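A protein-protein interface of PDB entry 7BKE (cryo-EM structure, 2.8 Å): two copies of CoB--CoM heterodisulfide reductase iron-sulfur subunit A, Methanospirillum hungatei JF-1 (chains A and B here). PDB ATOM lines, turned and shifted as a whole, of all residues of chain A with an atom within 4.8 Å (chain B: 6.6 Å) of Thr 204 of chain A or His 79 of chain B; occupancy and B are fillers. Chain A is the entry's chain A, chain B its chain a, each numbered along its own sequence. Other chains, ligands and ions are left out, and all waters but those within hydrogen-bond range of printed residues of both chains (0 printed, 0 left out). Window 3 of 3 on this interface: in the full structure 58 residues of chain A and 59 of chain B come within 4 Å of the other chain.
The side-chain amide nitrogen of Gln 200 of chain A sits at hydrogen-bond distance from the side-chain hydroxyl of Thr 204 of chain A, at 2.9 Å.
A ring nitrogen (ND1) of His 79 of chain B lies within hydrogen-bond range of the side-chain hydroxyl of Thr 82 of chain B (2.8 Å).
Among the printed residues, pairs that only touch across the chains: Cys 201 of chain A with Leu 78 of chain B, Ile 202 of chain A with Leu 541 of chain B, Thr 204 of chain A with His 79 of chain B and Lys 206 of chain A with Leu 541 of chain B.
Of the printed residues of chain B, Ile 202 of chain A touches Leu 541 (3.2 Å).
Of chain B, only His 79 comes within 4 Å of Thr 204 of chain A.
Of the printed residues of chain B, Lys 206 of chain A touches Leu 541.
His 79 of chain B touches one residue of chain A.
Of the printed residues of chain A, Leu 541 of chain B touches Ile 202 and Lys 206.
Of the 16 printed residues of chain B, 3 touch a printed residue of chain A.
Hydrophobic or aromatic side chains of chain B within 4 Å of the printed part of chain A: Leu 78, His 79 and Leu 541.
Along chain A the printed residues that touch a printed residue of chain B span positions 201 to 206.
Among the printed residues, no Asp or Glu carboxylate lies within 4 Å of a Lys or Arg side-chain nitrogen of the other chain.
No position is printed for both chains.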
ATOM      1  N   GLN A 200       5.536  23.507 -25.697  1.00  0.00           N
ATOM      2  CA  GLN A 200       5.461  23.462 -24.226  1.00  0.00           C
ATOM      3  C   GLN A 200       4.275  22.610 -23.823  1.00  0.00           C
ATOM      4  O   GLN A 200       4.398  21.865 -22.861  1.00  0.00           O
ATOM      5  CB  GLN A 200       5.398  24.869 -23.622  1.00  0.00           C
ATOM      6  CG  GLN A 200       5.834  24.938 -22.167  1.00  0.00           C
ATOM      7  CD  GLN A 200       7.177  24.289 -21.940  1.00  0.00           C
ATOM      8  OE1 GLN A 200       8.216  24.827 -22.310  1.00  0.00           O
ATOM      9  NE2 GLN A 200       7.165  23.126 -21.312  1.00  0.00           N
ATOM     10  N   CYS A 201       3.173  22.723 -24.552  1.00  0.00           N
ATOM     11  CA  CYS A 201       1.953  21.972 -24.203  1.00  0.00           C
ATOM     12  C   CYS A 201       2.240  20.474 -24.286  1.00  0.00           C
ATOM     13  O   CYS A 201       1.907  19.784 -23.341  1.00  0.00           O
ATOM     14  CB  CYS A 201       0.831  22.330 -25.169  1.00  0.00           C
ATOM     15  SG  CYS A 201       0.539  24.107 -25.403  1.00  0.00           S
ATOM     16  N   ILE A 202       2.878  20.009 -25.355  1.00  0.00           N
ATOM     17  CA  ILE A 202       3.206  18.563 -25.520  1.00  0.00           C
ATOM     18  C   ILE A 202       4.315  18.112 -24.567  1.00  0.00           C
ATOM     19  O   ILE A 202       4.355  16.927 -24.246  1.00  0.00           O
ATOM     20  CB  ILE A 202       3.406  18.132 -26.995  1.00  0.00           C
ATOM     21  CG1 ILE A 202       4.697  18.648 -27.628  1.00  0.00           C
ATOM     22  CG2 ILE A 202       2.187  18.497 -27.824  1.00  0.00           C
ATOM     23  CD1 ILE A 202       4.852  18.237 -29.074  1.00  0.00           C
ATOM     24  N   LEU A 203       5.192  19.009 -24.144  1.00  0.00           N
ATOM     25  CA  LEU A 203       6.328  18.612 -23.282  1.00  0.00           C
ATOM     26  C   LEU A 203       6.017  18.815 -21.798  1.00  0.00           C
ATOM     27  O   LEU A 203       6.585  18.075 -21.014  1.00  0.00           O
ATOM     28  CB  LEU A 203       7.584  19.393 -23.689  1.00  0.00           C
ATOM     29  CG  LEU A 203       8.908  18.886 -23.120  1.00  0.00           C
ATOM     30  CD1 LEU A 203       9.267  17.535 -23.714  1.00  0.00           C
ATOM     31  CD2 LEU A 203      10.017  19.893 -23.363  1.00  0.00           C
ATOM     32  N   THR A 204       5.155  19.766 -21.427  1.00  0.00           N
ATOM     33  CA  THR A 204       4.942  20.042 -19.979  1.00  0.00           C
ATOM     34  C   THR A 204       4.512  18.759 -19.277  1.00  0.00           C
ATOM     35  O   THR A 204       5.075  18.480 -18.218  1.00  0.00           O
ATOM     36  CB  THR A 204       4.019  21.236 -19.709  1.00  0.00           C
ATOM     37  OG1 THR A 204       4.835  22.404 -19.665  1.00  0.00           O
ATOM     38  CG2 THR A 204       3.235  21.117 -18.421  1.00  0.00           C
ATOM     39  N   PRO A 205       3.574  17.947 -19.798  1.00  0.00           N
ATOM     40  CA  PRO A 205       3.268  16.666 -19.189  1.00  0.00           C
ATOM     41  C   PRO A 205       4.508  15.834 -18.837  1.00  0.00           C
ATOM     42  O   PRO A 205       4.559  15.385 -17.731  1.00  0.00           O
ATOM     43  CB  PRO A 205       2.377  15.977 -20.223  1.00  0.00           C
ATOM     44  CG  PRO A 205       2.408  16.861 -21.441  1.00  0.00           C
ATOM     45  CD  PRO A 205       2.637  18.243 -20.882  1.00  0.00           C
ATOM     46  N   LYS A 206       5.442  15.631 -19.768  1.00  0.00           N
ATOM     47  CA  LYS A 206       6.629  14.816 -19.550  1.00  0.00           C
ATOM     48  C   LYS A 206       7.582  15.461 -18.554  1.00  0.00           C
ATOM     49  O   LYS A 206       8.242  14.756 -17.783  1.00  0.00           O
ATOM     50  CB  LYS A 206       7.331  14.540 -20.877  1.00  0.00           C
ATOM     51  CG  LYS A 206       6.429  13.855 -21.871  1.00  0.00           C
ATOM     52  CD  LYS A 206       7.207  13.080 -22.905  1.00  0.00           C
ATOM     53  CE  LYS A 206       7.534  11.695 -22.391  1.00  0.00           C
ATOM     54  NZ  LYS A 206       6.305  10.952 -22.006  1.00  0.00           N
ATOM     55  N   MET A 207       7.656  16.792 -18.540  1.00  0.00           N
ATOM     56  CA  MET A 207       8.432  17.465 -17.509  1.00  0.00           C
ATOM     57  C   MET A 207       7.858  17.184 -16.130  1.00  0.00           C
ATOM     58  O   MET A 207       8.605  16.942 -15.176  1.00  0.00           O
ATOM     59  CB  MET A 207       8.477  18.967 -17.782  1.00  0.00           C
ATOM     60  CG  MET A 207       9.561  19.374 -18.757  1.00  0.00           C
ATOM     61  SD  MET A 207       9.234  20.921 -19.614  1.00  0.00           S
ATOM     62  CE  MET A 207       9.756  22.104 -18.386  1.00  0.00           C
ATOM     63  N   VAL A 208       6.530  17.182 -16.009  1.00  0.00           N
ATOM     64  CA  VAL A 208       5.896  16.879 -14.729  1.00  0.00           C
ATOM     65  C   VAL A 208       6.168  15.436 -14.325  1.00  0.00           C
ATOM     66  O   VAL A 208       6.427  15.143 -13.153  1.00  0.00           O
ATOM     67  CB  VAL A 208       4.388  17.182 -14.797  1.00  0.00           C
ATOM     68  CG1 VAL A 208       3.704  16.737 -13.530  1.00  0.00           C
ATOM     69  CG2 VAL A 208       4.165  18.656 -15.011  1.00  0.00           C
ATOM     70  N   GLN A 295       7.245  28.144 -16.950  1.00  0.00           N
ATOM     71  CA  GLN A 295       6.976  26.714 -17.009  1.00  0.00           C
ATOM     72  C   GLN A 295       8.213  25.872 -16.719  1.00  0.00           C
ATOM     73  O   GLN A 295       8.303  24.729 -17.166  1.00  0.00           O
ATOM     74  CB  GLN A 295       6.402  26.320 -18.369  1.00  0.00           C
ATOM     75  CG  GLN A 295       4.949  26.672 -18.585  1.00  0.00           C
ATOM     76  CD  GLN A 295       4.754  28.096 -19.045  1.00  0.00           C
ATOM     77  OE1 GLN A 295       5.592  28.653 -19.751  1.00  0.00           O
ATOM     78  NE2 GLN A 295       3.646  28.695 -18.644  1.00  0.00           N
ATOM     79  N   CYS B  49      -1.607  24.363 -13.934  1.00  0.00           N
ATOM     80  CA  CYS B  49      -0.825  23.158 -14.150  1.00  0.00           C
ATOM     81  C   CYS B  49       0.537  23.224 -13.483  1.00  0.00           C
ATOM     82  O   CYS B  49       1.292  22.251 -13.547  1.00  0.00           O
ATOM     83  CB  CYS B  49      -0.666  22.889 -15.648  1.00  0.00           C
ATOM     84  SG  CYS B  49       0.065  24.236 -16.583  1.00  0.00           S
ATOM     85  N   CYS B  74      -7.501  23.915 -19.804  1.00  0.00           N
ATOM     86  CA  CYS B  74      -7.251  23.342 -21.118  1.00  0.00           C
ATOM     87  C   CYS B  74      -7.928  21.977 -21.254  1.00  0.00           C
ATOM     88  O   CYS B  74      -8.811  21.599 -20.481  1.00  0.00           O
ATOM     89  CB  CYS B  74      -5.751  23.233 -21.353  1.00  0.00           C
ATOM     90  SG  CYS B  74      -4.872  22.378 -20.039  1.00  0.00           S
ATOM     91  N   SER B  75      -7.556  21.251 -22.292  1.00  0.00           N
ATOM     92  CA  SER B  75      -8.255  20.034 -22.662  1.00  0.00           C
ATOM     93  C   SER B  75      -7.972  18.890 -21.689  1.00  0.00           C
ATOM     94  O   SER B  75      -6.856  18.769 -21.160  1.00  0.00           O
ATOM     95  CB  SER B  75      -7.857  19.616 -24.069  1.00  0.00           C
ATOM     96  OG  SER B  75      -8.164  18.258 -24.303  1.00  0.00           O
ATOM     97  N   PRO B  76      -8.960  18.024 -21.446  1.00  0.00           N
ATOM     98  CA  PRO B  76      -8.688  16.793 -20.699  1.00  0.00           C
ATOM     99  C   PRO B  76      -7.628  15.929 -21.339  1.00  0.00           C
ATOM    100  O   PRO B  76      -6.784  15.382 -20.623  1.00  0.00           O
ATOM    101  CB  PRO B  76     -10.048  16.091 -20.689  1.00  0.00           C
ATOM    102  CG  PRO B  76     -11.026  17.140 -20.964  1.00  0.00           C
ATOM    103  CD  PRO B  76     -10.369  18.125 -21.843  1.00  0.00           C
ATOM    104  N   ARG B  77      -7.628  15.816 -22.668  1.00  0.00           N
ATOM    105  CA  ARG B  77      -6.616  15.022 -23.349  1.00  0.00           C
ATOM    106  C   ARG B  77      -5.220  15.547 -23.079  1.00  0.00           C
ATOM    107  O   ARG B  77      -4.246  14.805 -23.231  1.00  0.00           O
ATOM    108  CB  ARG B  77      -6.876  15.004 -24.852  1.00  0.00           C
ATOM    109  CG  ARG B  77      -8.325  14.795 -25.229  1.00  0.00           C
ATOM    110  CD  ARG B  77      -8.573  15.185 -26.673  1.00  0.00           C
ATOM    111  NE  ARG B  77      -7.574  14.640 -27.586  1.00  0.00           N
ATOM    112  CZ  ARG B  77      -7.437  13.347 -27.873  1.00  0.00           C
ATOM    113  NH1 ARG B  77      -8.239  12.449 -27.328  1.00  0.00           N
ATOM    114  NH2 ARG B  77      -6.494  12.953 -28.715  1.00  0.00           N
ATOM    115  N   LEU B  78      -5.102  16.784 -22.614  1.00  0.00           N
ATOM    116  CA  LEU B  78      -3.761  17.285 -22.260  1.00  0.00           C
ATOM    117  C   LEU B  78      -3.487  17.139 -20.772  1.00  0.00           C
ATOM    118  O   LEU B  78      -2.399  16.708 -20.435  1.00  0.00           O
ATOM    119  CB  LEU B  78      -3.729  18.765 -22.630  1.00  0.00           C
ATOM    120  CG  LEU B  78      -2.351  19.424 -22.681  1.00  0.00           C
ATOM    121  CD1 LEU B  78      -1.436  18.691 -23.649  1.00  0.00           C
ATOM    122  CD2 LEU B  78      -2.475  20.887 -23.069  1.00  0.00           C
ATOM    123  N   HIS B  79      -4.456  17.420 -19.915  1.00  0.00           N
ATOM    124  CA  HIS B  79      -4.099  17.465 -18.500  1.00  0.00           C
ATOM    125  C   HIS B  79      -5.112  16.751 -17.607  1.00  0.00           C
ATOM    126  O   HIS B  79      -5.507  17.266 -16.563  1.00  0.00           O
ATOM    127  CB  HIS B  79      -3.927  18.911 -18.048  1.00  0.00           C
ATOM    128  CG  HIS B  79      -2.564  19.466 -18.312  1.00  0.00           C
ATOM    129  ND1 HIS B  79      -1.416  18.893 -17.813  1.00  0.00           N
ATOM    130  CD2 HIS B  79      -2.165  20.542 -19.029  1.00  0.00           C
ATOM    131  CE1 HIS B  79      -0.369  19.591 -18.210  1.00  0.00           C
ATOM    132  NE2 HIS B  79      -0.797  20.597 -18.950  1.00  0.00           N
ATOM    133  N   GLU B  80      -5.551  15.543 -17.986  1.00  0.00           N
ATOM    134  CA  GLU B  80      -6.149  14.674 -16.970  1.00  0.00           C
ATOM    135  C   GLU B  80      -5.121  14.082 -16.022  1.00  0.00           C
ATOM    136  O   GLU B  80      -5.354  14.122 -14.804  1.00  0.00           O
ATOM    137  CB  GLU B  80      -7.001  13.569 -17.605  1.00  0.00           C
ATOM    138  CG  GLU B  80      -8.245  14.016 -18.299  1.00  0.00           C
ATOM    139  CD  GLU B  80      -9.255  14.585 -17.320  1.00  0.00           C
ATOM    140  OE1 GLU B  80      -9.287  14.123 -16.165  1.00  0.00           O
ATOM    141  OE2 GLU B  80     -10.026  15.485 -17.698  1.00  0.00           O
ATOM    142  N   PRO B  81      -4.021  13.479 -16.478  1.00  0.00           N
ATOM    143  CA  PRO B  81      -3.098  12.875 -15.503  1.00  0.00           C
ATOM    144  C   PRO B  81      -2.581  13.858 -14.471  1.00  0.00           C
ATOM    145  O   PRO B  81      -2.511  13.523 -13.281  1.00  0.00           O
ATOM    146  CB  PRO B  81      -1.975  12.330 -16.391  1.00  0.00           C
ATOM    147  CG  PRO B  81      -2.622  12.102 -17.694  1.00  0.00           C
ATOM    148  CD  PRO B  81      -3.582  13.221 -17.858  1.00  0.00           C
ATOM    149  N   THR B  82      -2.268  15.084 -14.890  1.00  0.00           N
ATOM    150  CA  THR B  82      -1.724  16.074 -13.970  1.00  0.00           C
ATOM    151  C   THR B  82      -2.690  16.352 -12.833  1.00  0.00           C
ATOM    152  O   THR B  82      -2.337  16.243 -11.653  1.00  0.00           O
ATOM    153  CB  THR B  82      -1.413  17.365 -14.725  1.00  0.00           C
ATOM    154  OG1 THR B  82      -0.526  17.087 -15.812  1.00  0.00           O
ATOM    155  CG2 THR B  82      -0.773  18.380 -13.803  1.00  0.00           C
ATOM    156  N   PHE B  83      -3.925  16.685 -13.164  1.00  0.00           N
ATOM    157  CA  PHE B  83      -4.868  17.086 -12.138  1.00  0.00           C
ATOM    158  C   PHE B  83      -5.480  15.907 -11.411  1.00  0.00           C
ATOM    159  O   PHE B  83      -5.920  16.066 -10.274  1.00  0.00           O
ATOM    160  CB  PHE B  83      -5.956  17.942 -12.748  1.00  0.00           C
ATOM    161  CG  PHE B  83      -5.495  19.303 -13.138  1.00  0.00           C
ATOM    162  CD1 PHE B  83      -5.227  20.251 -12.180  1.00  0.00           C
ATOM    163  CD2 PHE B  83      -5.337  19.635 -14.463  1.00  0.00           C
ATOM    164  CE1 PHE B  83      -4.813  21.494 -12.533  1.00  0.00           C
ATOM    165  CE2 PHE B  83      -4.923  20.882 -14.818  1.00  0.00           C
ATOM    166  CZ  PHE B  83      -4.665  21.812 -13.853  1.00  0.00           C
ATOM    167  N   ARG B  84      -5.493  14.722 -12.013  1.00  0.00           N
ATOM    168  CA  ARG B  84      -5.873  13.536 -11.258  1.00  0.00           C
ATOM    169  C   ARG B  84      -4.839  13.225 -10.189  1.00  0.00           C
ATOM    170  O   ARG B  84      -5.194  12.860  -9.064  1.00  0.00           O
ATOM    171  CB  ARG B  84      -6.052  12.346 -12.192  1.00  0.00           C
ATOM    172  CG  ARG B  84      -7.360  12.349 -12.934  1.00  0.00           C
ATOM    173  CD  ARG B  84      -7.614  11.011 -13.564  1.00  0.00           C
ATOM    174  NE  ARG B  84      -8.900  10.978 -14.244  1.00  0.00           N
ATOM    175  CZ  ARG B  84      -9.114  10.336 -15.381  1.00  0.00           C
ATOM    176  NH1 ARG B  84      -8.127   9.671 -15.955  1.00  0.00           N
ATOM    177  NH2 ARG B  84     -10.309  10.354 -15.942  1.00  0.00           N
ATOM    178  N   PHE B  97     -12.646  13.964 -10.108  1.00  0.00           N
ATOM    179  CA  PHE B  97     -12.176  15.162 -10.781  1.00  0.00           C
ATOM    180  C   PHE B  97     -12.759  15.242 -12.185  1.00  0.00           C
ATOM    181  O   PHE B  97     -12.916  14.224 -12.860  1.00  0.00           O
ATOM    182  CB  PHE B  97     -10.656  15.162 -10.850  1.00  0.00           C
ATOM    183  CG  PHE B  97     -10.111  16.175 -11.778  1.00  0.00           C
ATOM    184  CD1 PHE B  97     -10.062  17.497 -11.409  1.00  0.00           C
ATOM    185  CD2 PHE B  97      -9.665  15.820 -13.028  1.00  0.00           C
ATOM    186  CE1 PHE B  97      -9.584  18.434 -12.254  1.00  0.00           C
ATOM    187  CE2 PHE B  97      -9.184  16.760 -13.880  1.00  0.00           C
ATOM    188  CZ  PHE B  97      -9.147  18.069 -13.485  1.00  0.00           C
ATOM    189  N   MET B  99     -12.850  18.127 -15.744  1.00  0.00           N
ATOM    190  CA  MET B  99     -12.397  19.373 -16.342  1.00  0.00           C
ATOM    191  C   MET B  99     -13.503  20.030 -17.153  1.00  0.00           C
ATOM    192  O   MET B  99     -14.431  19.378 -17.636  1.00  0.00           O
ATOM    193  CB  MET B  99     -11.186  19.159 -17.252  1.00  0.00           C
ATOM    194  CG  MET B  99      -9.915  18.941 -16.502  1.00  0.00           C
ATOM    195  SD  MET B  99      -8.400  18.947 -17.463  1.00  0.00           S
ATOM    196  CE  MET B  99      -8.137  20.699 -17.624  1.00  0.00           C
ATOM    197  N   ARG B 103     -10.549  26.643 -22.913  1.00  0.00           N
ATOM    198  CA  ARG B 103      -9.478  27.311 -23.678  1.00  0.00           C
ATOM    199  C   ARG B 103      -9.555  26.872 -25.119  1.00  0.00           C
ATOM    200  O   ARG B 103      -9.932  27.678 -25.954  1.00  0.00           O
ATOM    201  CB  ARG B 103      -8.081  26.914 -23.190  1.00  0.00           C
ATOM    202  CG  ARG B 103      -6.948  27.691 -23.839  1.00  0.00           C
ATOM    203  CD  ARG B 103      -5.620  27.253 -23.271  1.00  0.00           C
ATOM    204  NE  ARG B 103      -5.266  25.900 -23.650  1.00  0.00           N
ATOM    205  CZ  ARG B 103      -4.039  25.407 -23.617  1.00  0.00           C
ATOM    206  NH1 ARG B 103      -3.030  26.163 -23.237  1.00  0.00           N
ATOM    207  NH2 ARG B 103      -3.813  24.166 -23.995  1.00  0.00           N
ATOM    208  N   LEU B 541       6.293  12.786 -29.631  1.00  0.00           N
ATOM    209  CA  LEU B 541       6.880  12.278 -28.399  1.00  0.00           C
ATOM    210  C   LEU B 541       6.620  10.799 -28.163  1.00  0.00           C
ATOM    211  O   LEU B 541       6.936  10.298 -27.083  1.00  0.00           O
ATOM    212  CB  LEU B 541       6.377  13.091 -27.211  1.00  0.00           C
ATOM    213  CG  LEU B 541       6.887  14.526 -27.207  1.00  0.00           C
ATOM    214  CD1 LEU B 541       6.393  15.264 -25.995  1.00  0.00           C
ATOM    215  CD2 LEU B 541       8.399  14.537 -27.262  1.00  0.00           C
